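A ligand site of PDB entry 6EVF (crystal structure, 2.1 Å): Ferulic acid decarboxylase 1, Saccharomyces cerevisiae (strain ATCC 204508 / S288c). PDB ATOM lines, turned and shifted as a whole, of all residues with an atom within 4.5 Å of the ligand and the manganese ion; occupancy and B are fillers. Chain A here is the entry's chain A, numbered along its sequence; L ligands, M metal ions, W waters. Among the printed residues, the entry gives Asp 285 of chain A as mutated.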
ATOM      1  N   GLN A 154       0.421  10.150  28.088  1.00  0.00           N
ATOM      2  CA  GLN A 154       1.615   9.802  27.319  1.00  0.00           C
ATOM      3  C   GLN A 154       2.798  10.803  27.533  1.00  0.00           C
ATOM      4  O   GLN A 154       2.894  11.832  26.855  1.00  0.00           O
ATOM      5  CB  GLN A 154       1.235   9.513  25.876  1.00  0.00           C
ATOM      6  CG  GLN A 154       2.297   9.557  24.822  1.00  0.00           C
ATOM      7  CD  GLN A 154       3.523   8.687  25.089  1.00  0.00           C
ATOM      8  OE1 GLN A 154       3.773   8.308  26.182  1.00  0.00           O
ATOM      9  NE2 GLN A 154       4.289   8.382  24.032  1.00  0.00           N
ATOM     10  N   THR A 155       3.658  10.514  28.506  1.00  0.00           N
ATOM     11  CA  THR A 155       4.936  11.189  28.627  1.00  0.00           C
ATOM     12  C   THR A 155       6.167  10.247  28.512  1.00  0.00           C
ATOM     13  O   THR A 155       7.266  10.729  28.334  1.00  0.00           O
ATOM     14  CB  THR A 155       5.002  11.963  29.944  1.00  0.00           C
ATOM     15  OG1 THR A 155       4.810  11.055  31.041  1.00  0.00           O
ATOM     16  CG2 THR A 155       3.927  13.071  29.990  1.00  0.00           C
ATOM     17  N   TYR A 156       6.018   8.932  28.690  1.00  0.00           N
ATOM     18  CA  TYR A 156       7.168   8.004  28.574  1.00  0.00           C
ATOM     19  C   TYR A 156       6.762   6.624  28.093  1.00  0.00           C
ATOM     20  O   TYR A 156       7.263   5.591  28.582  1.00  0.00           O
ATOM     21  CB  TYR A 156       7.818   7.927  29.915  1.00  0.00           C
ATOM     22  CG  TYR A 156       9.266   7.572  29.933  1.00  0.00           C
ATOM     23  CD1 TYR A 156      10.226   8.500  29.618  1.00  0.00           C
ATOM     24  CD2 TYR A 156       9.694   6.321  30.356  1.00  0.00           C
ATOM     25  CE1 TYR A 156      11.567   8.172  29.641  1.00  0.00           C
ATOM     26  CE2 TYR A 156      11.048   6.005  30.455  1.00  0.00           C
ATOM     27  CZ  TYR A 156      11.983   6.963  30.106  1.00  0.00           C
ATOM     28  OH  TYR A 156      13.333   6.727  30.148  1.00  0.00           O
ATOM     29  N   TRP A 168       8.941   0.006   7.245  1.00  0.00           N
ATOM     30  CA  TRP A 168       9.568   0.838   8.239  1.00  0.00           C
ATOM     31  C   TRP A 168       8.599   0.910   9.386  1.00  0.00           C
ATOM     32  O   TRP A 168       7.438   1.312   9.167  1.00  0.00           O
ATOM     33  CB  TRP A 168       9.955   2.221   7.642  1.00  0.00           C
ATOM     34  CG  TRP A 168      10.478   3.242   8.633  1.00  0.00           C
ATOM     35  CD1 TRP A 168      11.086   2.999   9.868  1.00  0.00           C
ATOM     36  CD2 TRP A 168      10.359   4.658   8.535  1.00  0.00           C
ATOM     37  NE1 TRP A 168      11.377   4.181  10.495  1.00  0.00           N
ATOM     38  CE2 TRP A 168      10.937   5.210   9.711  1.00  0.00           C
ATOM     39  CE3 TRP A 168       9.896   5.531   7.535  1.00  0.00           C
ATOM     40  CZ2 TRP A 168      11.064   6.583   9.911  1.00  0.00           C
ATOM     41  CZ3 TRP A 168      10.032   6.876   7.725  1.00  0.00           C
ATOM     42  CH2 TRP A 168      10.594   7.397   8.936  1.00  0.00           C
ATOM     43  N   ASN A 170       8.398   2.613  13.082  1.00  0.00           N
ATOM     44  CA  ASN A 170       9.004   3.629  13.893  1.00  0.00           C
ATOM     45  C   ASN A 170       8.475   3.536  15.306  1.00  0.00           C
ATOM     46  O   ASN A 170       7.255   3.458  15.514  1.00  0.00           O
ATOM     47  CB  ASN A 170       8.720   5.005  13.330  1.00  0.00           C
ATOM     48  CG  ASN A 170       9.649   6.075  13.895  1.00  0.00           C
ATOM     49  OD1 ASN A 170       9.286   6.790  14.835  1.00  0.00           O
ATOM     50  ND2 ASN A 170      10.795   6.206  13.327  1.00  0.00           N
ATOM     51  N   TRP A 171       9.406   3.568  16.277  1.00  0.00           N
ATOM     52  CA  TRP A 171       9.111   3.709  17.701  1.00  0.00           C
ATOM     53  C   TRP A 171       9.553   5.078  18.177  1.00  0.00           C
ATOM     54  O   TRP A 171      10.721   5.416  18.031  1.00  0.00           O
ATOM     55  CB  TRP A 171       9.825   2.636  18.489  1.00  0.00           C
ATOM     56  CG  TRP A 171       9.370   1.204  18.212  1.00  0.00           C
ATOM     57  CD1 TRP A 171       8.329   0.797  17.420  1.00  0.00           C
ATOM     58  CD2 TRP A 171       9.935  -0.004  18.790  1.00  0.00           C
ATOM     59  NE1 TRP A 171       8.194  -0.579  17.479  1.00  0.00           N
ATOM     60  CE2 TRP A 171       9.183  -1.102  18.284  1.00  0.00           C
ATOM     61  CE3 TRP A 171      11.004  -0.248  19.636  1.00  0.00           C
ATOM     62  CZ2 TRP A 171       9.446  -2.415  18.635  1.00  0.00           C
ATOM     63  CZ3 TRP A 171      11.284  -1.547  19.990  1.00  0.00           C
ATOM     64  CH2 TRP A 171      10.502  -2.623  19.496  1.00  0.00           C
ATOM     65  N   SER A 172       8.666   5.851  18.784  1.00  0.00           N
ATOM     66  CA  SER A 172       9.030   7.192  19.230  1.00  0.00           C
ATOM     67  C   SER A 172       8.151   7.690  20.326  1.00  0.00           C
ATOM     68  O   SER A 172       7.077   7.183  20.566  1.00  0.00           O
ATOM     69  CB  SER A 172       8.984   8.202  18.069  1.00  0.00           C
ATOM     70  OG  SER A 172       7.664   8.370  17.579  1.00  0.00           O
ATOM     71  N   ILE A 173       8.690   8.661  21.031  1.00  0.00           N
ATOM     72  CA  ILE A 173       7.956   9.334  22.092  1.00  0.00           C
ATOM     73  C   ILE A 173       7.501  10.703  21.519  1.00  0.00           C
ATOM     74  O   ILE A 173       8.296  11.471  20.934  1.00  0.00           O
ATOM     75  CB  ILE A 173       8.838   9.606  23.307  1.00  0.00           C
ATOM     76  CG1 ILE A 173       9.498   8.332  23.824  1.00  0.00           C
ATOM     77  CG2 ILE A 173       8.070  10.319  24.405  1.00  0.00           C
ATOM     78  CD1 ILE A 173      10.120   8.505  25.198  1.00  0.00           C
ATOM     79  N   ALA A 174       6.232  10.991  21.769  1.00  0.00           N
ATOM     80  CA  ALA A 174       5.567  12.263  21.562  1.00  0.00           C
ATOM     81  C   ALA A 174       4.438  12.390  22.600  1.00  0.00           C
ATOM     82  O   ALA A 174       3.756  11.389  22.960  1.00  0.00           O
ATOM     83  CB  ALA A 174       4.966  12.312  20.176  1.00  0.00           C
ATOM     84  N   ARG A 175       4.232  13.606  23.093  1.00  0.00           N
ATOM     85  CA  ARG A 175       3.295  13.801  24.174  1.00  0.00           C
ATOM     86  C   ARG A 175       1.858  13.555  23.740  1.00  0.00           C
ATOM     87  O   ARG A 175       1.506  13.824  22.597  1.00  0.00           O
ATOM     88  CB  ARG A 175       3.412  15.147  24.767  1.00  0.00           C
ATOM     89  CG  ARG A 175       2.891  16.229  23.895  1.00  0.00           C
ATOM     90  CD  ARG A 175       3.282  17.541  24.512  1.00  0.00           C
ATOM     91  NE  ARG A 175       2.499  18.579  23.897  1.00  0.00           N
ATOM     92  CZ  ARG A 175       2.865  19.846  23.788  1.00  0.00           C
ATOM     93  NH1 ARG A 175       4.035  20.255  24.219  1.00  0.00           N
ATOM     94  NH2 ARG A 175       2.025  20.706  23.214  1.00  0.00           N
ATOM     95  N   LEU A 187       1.117  15.819  19.960  1.00  0.00           N
ATOM     96  CA  LEU A 187       1.969  16.351  18.871  1.00  0.00           C
ATOM     97  C   LEU A 187       2.349  15.270  17.875  1.00  0.00           C
ATOM     98  O   LEU A 187       2.886  14.236  18.278  1.00  0.00           O
ATOM     99  CB  LEU A 187       3.258  16.901  19.438  1.00  0.00           C
ATOM    100  CG  LEU A 187       3.235  18.169  20.300  1.00  0.00           C
ATOM    101  CD1 LEU A 187       4.658  18.667  20.580  1.00  0.00           C
ATOM    102  CD2 LEU A 187       2.435  19.268  19.631  1.00  0.00           C
ATOM    103  N   ILE A 189       4.228  16.280  14.639  1.00  0.00           N
ATOM    104  CA  ILE A 189       4.731  17.473  13.931  1.00  0.00           C
ATOM    105  C   ILE A 189       5.951  17.158  13.113  1.00  0.00           C
ATOM    106  O   ILE A 189       6.772  16.301  13.485  1.00  0.00           O
ATOM    107  CB  ILE A 189       5.082  18.629  14.893  1.00  0.00           C
ATOM    108  CG1 ILE A 189       6.168  18.240  15.924  1.00  0.00           C
ATOM    109  CG2 ILE A 189       3.829  19.090  15.607  1.00  0.00           C
ATOM    110  CD1 ILE A 189       6.995  19.405  16.473  1.00  0.00           C
ATOM    111  N   GLN A 192       9.310  15.162  12.723  1.00  0.00           N
ATOM    112  CA  GLN A 192       9.314  13.911  13.447  1.00  0.00           C
ATOM    113  C   GLN A 192       8.811  12.731  12.607  1.00  0.00           C
ATOM    114  O   GLN A 192       7.977  12.882  11.710  1.00  0.00           O
ATOM    115  CB  GLN A 192       8.521  14.034  14.754  1.00  0.00           C
ATOM    116  CG  GLN A 192       8.972  15.198  15.662  1.00  0.00           C
ATOM    117  CD  GLN A 192      10.356  14.941  16.247  1.00  0.00           C
ATOM    118  OE1 GLN A 192      11.363  15.037  15.529  1.00  0.00           O
ATOM    119  NE2 GLN A 192      10.409  14.498  17.513  1.00  0.00           N
ATOM    120  N   HIS A 193       9.389  11.552  12.842  1.00  0.00           N
ATOM    121  CA  HIS A 193       9.044  10.389  12.046  1.00  0.00           C
ATOM    122  C   HIS A 193       7.606   9.911  12.180  1.00  0.00           C
ATOM    123  O   HIS A 193       7.088   9.340  11.243  1.00  0.00           O
ATOM    124  CB  HIS A 193      10.015   9.264  12.221  1.00  0.00           C
ATOM    125  CG  HIS A 193      11.391   9.603  11.748  1.00  0.00           C
ATOM    126  ND1 HIS A 193      12.520   8.945  12.208  1.00  0.00           N
ATOM    127  CD2 HIS A 193      11.813  10.512  10.834  1.00  0.00           C
ATOM    128  CE1 HIS A 193      13.574   9.447  11.588  1.00  0.00           C
ATOM    129  NE2 HIS A 193      13.183  10.395  10.760  1.00  0.00           N
ATOM    130  N   ILE A 194       6.997  10.160  13.309  1.00  0.00           N
ATOM    131  CA  ILE A 194       5.623   9.872  13.543  1.00  0.00           C
ATOM    132  C   ILE A 194       4.734  10.653  12.539  1.00  0.00           C
ATOM    133  O   ILE A 194       3.840  10.053  11.980  1.00  0.00           O
ATOM    134  CB  ILE A 194       5.226  10.151  15.016  1.00  0.00           C
ATOM    135  CG1 ILE A 194       3.870   9.496  15.317  1.00  0.00           C
ATOM    136  CG2 ILE A 194       5.315  11.629  15.370  1.00  0.00           C
ATOM    137  CD1 ILE A 194       3.353   9.708  16.725  1.00  0.00           C
ATOM    138  N   SER A 226      13.480   5.070  21.447  1.00  0.00           N
ATOM    139  CA  SER A 226      12.293   5.879  21.104  1.00  0.00           C
ATOM    140  C   SER A 226      12.520   7.403  21.145  1.00  0.00           C
ATOM    141  O   SER A 226      11.916   8.151  20.322  1.00  0.00           O
ATOM    142  CB  SER A 226      11.071   5.472  21.940  1.00  0.00           C
ATOM    143  OG  SER A 226      10.736   4.102  21.700  1.00  0.00           O
ATOM    144  N   SER A 227      13.387   7.867  22.045  1.00  0.00           N
ATOM    145  CA  SER A 227      13.720   9.298  22.152  1.00  0.00           C
ATOM    146  C   SER A 227      14.905   9.742  21.303  1.00  0.00           C
ATOM    147  O   SER A 227      15.316  10.909  21.399  1.00  0.00           O
ATOM    148  CB  SER A 227      14.033   9.670  23.560  1.00  0.00           C
ATOM    149  OG  SER A 227      14.187  11.089  23.657  1.00  0.00           O
ATOM    150  N   MET A 228      15.461   8.837  20.510  1.00  0.00           N
ATOM    151  CA  MET A 228      16.647   9.106  19.758  1.00  0.00           C
ATOM    152  C   MET A 228      16.403   9.383  18.288  1.00  0.00           C
ATOM    153  O   MET A 228      15.679   8.628  17.647  1.00  0.00           O
ATOM    154  CB  MET A 228      17.570   7.904  19.911  1.00  0.00           C
ATOM    155  CG  MET A 228      18.880   8.057  19.228  1.00  0.00           C
ATOM    156  SD  MET A 228      19.881   6.606  19.678  1.00  0.00           S
ATOM    157  CE  MET A 228      21.409   7.100  18.907  1.00  0.00           C
ATOM    158  N   PRO A 229      17.043  10.415  17.715  1.00  0.00           N
ATOM    159  CA  PRO A 229      16.819  10.709  16.299  1.00  0.00           C
ATOM    160  C   PRO A 229      17.679   9.876  15.365  1.00  0.00           C
ATOM    161  O   PRO A 229      18.611  10.368  14.656  1.00  0.00           O
ATOM    162  CB  PRO A 229      17.086  12.243  16.223  1.00  0.00           C
ATOM    163  CG  PRO A 229      18.116  12.477  17.241  1.00  0.00           C
ATOM    164  CD  PRO A 229      17.811  11.506  18.372  1.00  0.00           C
ATOM    165  N   ILE A 230      17.369   8.597  15.324  1.00  0.00           N
ATOM    166  CA  ILE A 230      18.035   7.760  14.365  1.00  0.00           C
ATOM    167  C   ILE A 230      17.493   8.009  12.927  1.00  0.00           C
ATOM    168  O   ILE A 230      16.492   8.703  12.731  1.00  0.00           O
ATOM    169  CB  ILE A 230      17.984   6.269  14.768  1.00  0.00           C
ATOM    170  CG1 ILE A 230      16.595   5.686  14.632  1.00  0.00           C
ATOM    171  CG2 ILE A 230      18.505   6.033  16.147  1.00  0.00           C
ATOM    172  CD1 ILE A 230      16.572   4.170  14.874  1.00  0.00           C
ATOM    173  N   GLU A 236      13.441   1.408  14.655  1.00  0.00           N
ATOM    174  CA  GLU A 236      14.117   1.450  15.951  1.00  0.00           C
ATOM    175  C   GLU A 236      14.318   0.052  16.577  1.00  0.00           C
ATOM    176  O   GLU A 236      15.359  -0.198  17.194  1.00  0.00           O
ATOM    177  CB  GLU A 236      13.306   2.246  16.919  1.00  0.00           C
ATOM    178  CG  GLU A 236      13.499   3.722  16.855  1.00  0.00           C
ATOM    179  CD  GLU A 236      12.835   4.403  15.649  1.00  0.00           C
ATOM    180  OE1 GLU A 236      12.043   3.799  14.882  1.00  0.00           O
ATOM    181  OE2 GLU A 236      13.089   5.595  15.542  1.00  0.00           O
ATOM    182  N   PHE A 283       1.505  22.275  27.473  1.00  0.00           N
ATOM    183  CA  PHE A 283       2.136  21.300  28.352  1.00  0.00           C
ATOM    184  C   PHE A 283       3.424  21.877  28.900  1.00  0.00           C
ATOM    185  O   PHE A 283       4.188  22.469  28.175  1.00  0.00           O
ATOM    186  CB  PHE A 283       2.463  20.043  27.569  1.00  0.00           C
ATOM    187  CG  PHE A 283       2.989  18.914  28.421  1.00  0.00           C
ATOM    188  CD1 PHE A 283       2.272  18.488  29.546  1.00  0.00           C
ATOM    189  CD2 PHE A 283       4.210  18.324  28.141  1.00  0.00           C
ATOM    190  CE1 PHE A 283       2.754  17.463  30.343  1.00  0.00           C
ATOM    191  CE2 PHE A 283       4.670  17.292  28.904  1.00  0.00           C
ATOM    192  CZ  PHE A 283       3.953  16.861  30.002  1.00  0.00           C
ATOM    193  N   ASP A 285       6.959  22.087  29.478  1.00  0.00           N
ATOM    194  CA  ASP A 285       7.899  21.447  28.579  1.00  0.00           C
ATOM    195  C   ASP A 285       9.383  21.585  28.953  1.00  0.00           C
ATOM    196  O   ASP A 285       9.711  21.937  30.084  1.00  0.00           O
ATOM    197  CB  ASP A 285       7.573  21.713  27.106  1.00  0.00           C
ATOM    198  CG  ASP A 285       7.746  20.387  26.231  1.00  0.00           C
ATOM    199  OD1 ASP A 285       8.587  19.507  26.607  1.00  0.00           O
ATOM    200  OD2 ASP A 285       7.040  20.207  25.226  1.00  0.00           O
ATOM    201  N   SER A 317       7.320  11.052  32.724  1.00  0.00           N
ATOM    202  CA  SER A 317       8.251  12.176  32.805  1.00  0.00           C
ATOM    203  C   SER A 317       7.445  13.482  32.975  1.00  0.00           C
ATOM    204  O   SER A 317       6.387  13.692  32.351  1.00  0.00           O
ATOM    205  CB  SER A 317       9.093  12.240  31.528  1.00  0.00           C
ATOM    206  OG  SER A 317       9.949  13.388  31.476  1.00  0.00           O
ATOM    207  N   PRO A 319       8.252  17.195  32.628  1.00  0.00           N
ATOM    208  CA  PRO A 319       9.370  18.085  32.224  1.00  0.00           C
ATOM    209  C   PRO A 319       9.344  19.447  32.838  1.00  0.00           C
ATOM    210  O   PRO A 319       8.279  19.925  33.315  1.00  0.00           O
ATOM    211  CB  PRO A 319       9.212  18.209  30.701  1.00  0.00           C
ATOM    212  CG  PRO A 319       8.277  17.132  30.281  1.00  0.00           C
ATOM    213  CD  PRO A 319       7.360  16.909  31.481  1.00  0.00           C
ATOM    214  N   GLU A 325      14.072  14.015  31.867  1.00  0.00           N
ATOM    215  CA  GLU A 325      14.330  13.188  30.705  1.00  0.00           C
ATOM    216  C   GLU A 325      14.439  14.011  29.395  1.00  0.00           C
ATOM    217  O   GLU A 325      15.069  13.573  28.422  1.00  0.00           O
ATOM    218  CB  GLU A 325      13.218  12.172  30.507  1.00  0.00           C
ATOM    219  CG  GLU A 325      13.170  11.108  31.579  1.00  0.00           C
ATOM    220  CD  GLU A 325      12.535  11.500  32.920  1.00  0.00           C
ATOM    221  OE1 GLU A 325      11.747  12.511  32.993  1.00  0.00           O
ATOM    222  OE2 GLU A 325      12.897  10.774  33.888  1.00  0.00           O
ATOM    223  N   THR A 326      13.789  15.175  29.373  1.00  0.00           N
ATOM    224  CA  THR A 326      13.867  16.025  28.203  1.00  0.00           C
ATOM    225  C   THR A 326      15.307  16.609  28.051  1.00  0.00           C
ATOM    226  O   THR A 326      15.639  17.191  27.018  1.00  0.00           O
ATOM    227  CB  THR A 326      12.778  17.138  28.220  1.00  0.00           C
ATOM    228  OG1 THR A 326      13.010  18.065  29.283  1.00  0.00           O
ATOM    229  CG2 THR A 326      11.375  16.559  28.313  1.00  0.00           C
ATOM    230  N   LEU A 329      17.641  12.537  28.122  1.00  0.00           N
ATOM    231  CA  LEU A 329      17.428  11.724  26.915  1.00  0.00           C
ATOM    232  C   LEU A 329      17.401  12.549  25.665  1.00  0.00           C
ATOM    233  O   LEU A 329      18.119  12.281  24.710  1.00  0.00           O
ATOM    234  CB  LEU A 329      16.163  10.838  27.012  1.00  0.00           C
ATOM    235  CG  LEU A 329      16.116   9.907  28.183  1.00  0.00           C
ATOM    236  CD1 LEU A 329      14.844   9.063  28.136  1.00  0.00           C
ATOM    237  CD2 LEU A 329      17.359   9.052  28.231  1.00  0.00           C
ATOM    238  N   ILE A 330      16.540  13.555  25.611  1.00  0.00           N
ATOM    239  CA  ILE A 330      16.379  14.312  24.361  1.00  0.00           C
ATOM    240  C   ILE A 330      17.734  14.908  24.035  1.00  0.00           C
ATOM    241  O   ILE A 330      18.255  14.649  22.967  1.00  0.00           O
ATOM    242  CB  ILE A 330      15.281  15.388  24.370  1.00  0.00           C
ATOM    243  CG1 ILE A 330      13.924  14.795  24.674  1.00  0.00           C
ATOM    244  CG2 ILE A 330      15.149  16.045  23.009  1.00  0.00           C
ATOM    245  CD1 ILE A 330      12.802  15.798  24.582  1.00  0.00           C
ATOM    246  N   LYS A 394      17.441  17.409  10.737  1.00  0.00           N
ATOM    247  CA  LYS A 394      16.539  16.980  11.822  1.00  0.00           C
ATOM    248  C   LYS A 394      17.248  16.919  13.166  1.00  0.00           C
ATOM    249  O   LYS A 394      16.719  17.345  14.147  1.00  0.00           O
ATOM    250  CB  LYS A 394      15.897  15.636  11.504  1.00  0.00           C
ATOM    251  CG  LYS A 394      15.046  15.023  12.615  1.00  0.00           C
ATOM    252  CD  LYS A 394      14.184  13.926  11.960  1.00  0.00           C
ATOM    253  CE  LYS A 394      13.335  13.177  12.996  1.00  0.00           C
ATOM    254  NZ  LYS A 394      14.197  12.469  13.994  1.00  0.00           N
HETATM  255  C1  LIG L   1      11.147  12.845  24.193  1.00  0.00           C
HETATM  256  C2  LIG L   1      11.088  12.517  25.534  1.00  0.00           C
HETATM  257  C3  LIG L   1      10.062  12.976  26.380  1.00  0.00           C
HETATM  258  C4  LIG L   1       9.109  14.583  21.718  1.00  0.00           C
HETATM  259  C5  LIG L   1       9.080  13.916  25.880  1.00  0.00           C
HETATM  260  N1  LIG L   1       6.916  15.586  20.537  1.00  0.00           N
HETATM  261  C6  LIG L   1       7.906  15.133  19.804  1.00  0.00           C
HETATM  262  C7  LIG L   1       8.041  14.620  28.149  1.00  0.00           C
HETATM  263  C8  LIG L   1       7.929  14.483  26.616  1.00  0.00           C
HETATM  264  C9  LIG L   1       7.585  16.135  24.731  1.00  0.00           C
HETATM  265  O1  LIG L   1       7.680  15.179  18.513  1.00  0.00           O
HETATM  266  N2  LIG L   1       9.041  14.649  20.362  1.00  0.00           N
HETATM  267  C10 LIG L   1       6.948  15.530  21.898  1.00  0.00           C
HETATM  268  O2  LIG L   1       5.934  15.907  22.515  1.00  0.00           O
HETATM  269  C11 LIG L   1       8.054  15.058  22.547  1.00  0.00           C
HETATM  270  N3  LIG L   1       8.253  15.181  23.895  1.00  0.00           N
HETATM  271  C12 LIG L   1       7.473  15.781  26.085  1.00  0.00           C
HETATM  272  C13 LIG L   1       6.747  13.546  26.455  1.00  0.00           C
HETATM  273  C14 LIG L   1       9.176  14.250  24.495  1.00  0.00           C
HETATM  274  C15 LIG L   1      10.148  12.427  27.802  1.00  0.00           C
HETATM  275  C16 LIG L   1      12.158  11.588  25.987  1.00  0.00           C
HETATM  276  C17 LIG L   1      10.224  13.734  23.665  1.00  0.00           C
HETATM  277  N4  LIG L   1      10.287  14.105  22.303  1.00  0.00           N
HETATM  278  C18 LIG L   1      11.348  13.783  21.359  1.00  0.00           C
HETATM  279  C19 LIG L   1      11.261  12.591  20.435  1.00  0.00           C
HETATM  280  O3  LIG L   1      10.954  11.466  21.221  1.00  0.00           O
HETATM  281  C20 LIG L   1      12.606  12.541  19.745  1.00  0.00           C
HETATM  282  O4  LIG L   1      12.706  13.725  18.931  1.00  0.00           O
HETATM  283  C21 LIG L   1      12.771  11.319  18.866  1.00  0.00           C
HETATM  284  O5  LIG L   1      13.974  11.458  18.123  1.00  0.00           O
HETATM  285  C22 LIG L   1      11.599  11.165  17.922  1.00  0.00           C
HETATM  286  O6  LIG L   1      11.631   9.939  17.232  1.00  0.00           O
HETATM  287  P1  LIG L   1      11.866   9.891  15.641  1.00  0.00           P
HETATM  288  O7  LIG L   1      11.586   8.453  15.376  1.00  0.00           O
HETATM  289  O8  LIG L   1      10.824  10.800  15.054  1.00  0.00           O
HETATM  290  O9  LIG L   1      13.289  10.280  15.431  1.00  0.00           O
HETATM  291 MN    MN M   1      12.639   7.127  13.875  1.00  0.00          MN
HETATM  292  O   HOH W   1       5.451  14.864  17.063  1.00  0.00           O
HETATM  293  O   HOH W   2      13.861   5.942  12.223  1.00  0.00           O
HETATM  294  O   HOH W   3       8.399  10.559  16.002  1.00  0.00           O
HETATM  295  O   HOH W   4      14.613   8.300  14.555  1.00  0.00           O
HETATM  296  O   HOH W   5      15.088  14.736  19.518  1.00  0.00           O
HETATM  297  O   HOH W   6      13.775  14.181  16.176  1.00  0.00           O
HETATM  298  O   HOH W   7       8.108  12.222  18.356  1.00  0.00           O
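The backbone carbonyl oxygen (O) of Ile 173 is in hydrogen-bond range of an oxygen (O3) of the ligand (2.7 Å).
O9 of the ligand lies within salt-bridge range of NZ of Lys 394.
NE2 of Gln 192 lies within hydrogen-bond range of O4 of the ligand (2.8 Å).
The backbone NH (N) of Arg 175 lies within hydrogen-bond range of an oxygen (O2) of the ligand, at 2.9 Å.
O5 of the ligand sits close to O of Met 228 (3.3 Å).
The backbone NH of His 193 lies within hydrogen-bond range of an oxygen (O8) of the ligand (2.7 Å).
The side-chain hydroxyl (OG) of Ser 317 sits at hydrogen-bond distance from the side-chain carboxylate (OE1) of Glu 325 (2.5 Å).
N of Ser 317 sits at hydrogen-bond distance from OG1 of Thr 155 (3.0 Å).
NE2 of Gln 154 lies close to O of Ala 174, at 3.2 Å.
The backbone carbonyl oxygen (O) of Arg 175 sits at hydrogen-bond distance from the backbone NH (N) of Leu 187, at 3.3 Å.
N of Ile 173 sits at hydrogen-bond distance from O of Ser 226 (3.3 Å).
NH1 of Arg 175 is in salt-bridge range of OD2 of Asp 285, 3.2 Å away.
The backbone NH (N) of Ile 330 sits at hydrogen-bond distance from the backbone carbonyl oxygen (O) of Glu 325 (3.2 Å).
The side-chain carboxylate (OE1) of Glu 236 is in hydrogen-bond range of the backbone NH (N) of Trp 171.
Three residues have an atom within 4 Å of the manganese ion: Asn 170, His 193 and Glu 236.
The nearest printed residue that does not touch the manganese ion is Ile 230 (4.3 Å).
The manganese ion is bound by the side-chain amide nitrogen of Asn 170 (2.1 Å), an oxygen (O7) of the ligand (2.3 Å), the side-chain carboxylate of Glu 236 (2.3 Å), water W2 (2.4 Å), water W4 (2.4 Å) and a ring nitrogen (ND1) of His 193 (2.5 Å).
The manganese ion has six donor atoms within binding distance.
An oxygen (O5) of the ligand lies close to the backbone nitrogen (N) of Pro 229, 3.3 Å away.
Thr 155 touches the ligand (O to C15, 3.4 Å).
Ser 172 touches the ligand.
CA of Ala 174 touches C10 of the ligand (3.6 Å).
CD1 of Leu 187 touches O2 of the ligand (3.6 Å).
O of Ser 226 touches O3 of the ligand (3.6 Å).
OG of Ser 227 touches C16 of the ligand (3.1 Å).
Asp 285 touches the ligand (OD1 to C12, 3.9 Å).
Ser 317 touches the ligand.
Pro 319 touches the ligand (CG to C7, 3.3 Å).
Thr 326 touches the ligand (CG2 to C7, 3.9 Å).
Ile 330 touches the ligand.
Hydrophobic or aromatic side chains that line the ligand: Ile 173, Ala 174, Leu 187, His 193, Pro 229, Pro 319 and Ile 330.
20 residues have an atom within 4 Å of the ligand: Thr 155, Asn 170, Ser 172, Ile 173, Ala 174, Arg 175, Leu 187, Gln 192, His 193, Ser 226, Ser 227, Met 228, Pro 229, Glu 236, Asp 285, Ser 317, Pro 319, Thr 326, Ile 330 and Lys 394.
The nearest printed residue that does not touch the ligand is Glu 325 (4.1 Å).
Water W4 lies within hydrogen-bond range of an oxygen (O9) of the ligand (2.5 Å), the backbone carbonyl oxygen (O) of Ile 230 (2.6 Å) and the backbone carbonyl oxygen (O) of Met 228 (3.3 Å).
Water W3 lies within hydrogen-bond range of O8 of the ligand (2.6 Å), OG of Ser 172 (2.8 Å), N of Ile 194 (3.1 Å) and N of His 193 (3.5 Å).
Water W1 lies within hydrogen-bond range of O1 of the ligand (2.7 Å), O of Leu 187 (2.9 Å) and N of Ile 189 (3.1 Å).
Water W6 lies within hydrogen-bond range of OE1 of Gln 192 (2.6 Å), NZ of Lys 394 (2.8 Å) and O4 of the ligand (3.0 Å).
Water W7 lies within hydrogen-bond range of the backbone carbonyl oxygen (O) of Ile 173 (2.7 Å), an oxygen (O1) of the ligand (3.0 Å) and the side-chain amide nitrogen (NE2) of Gln 192 (3.3 Å).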
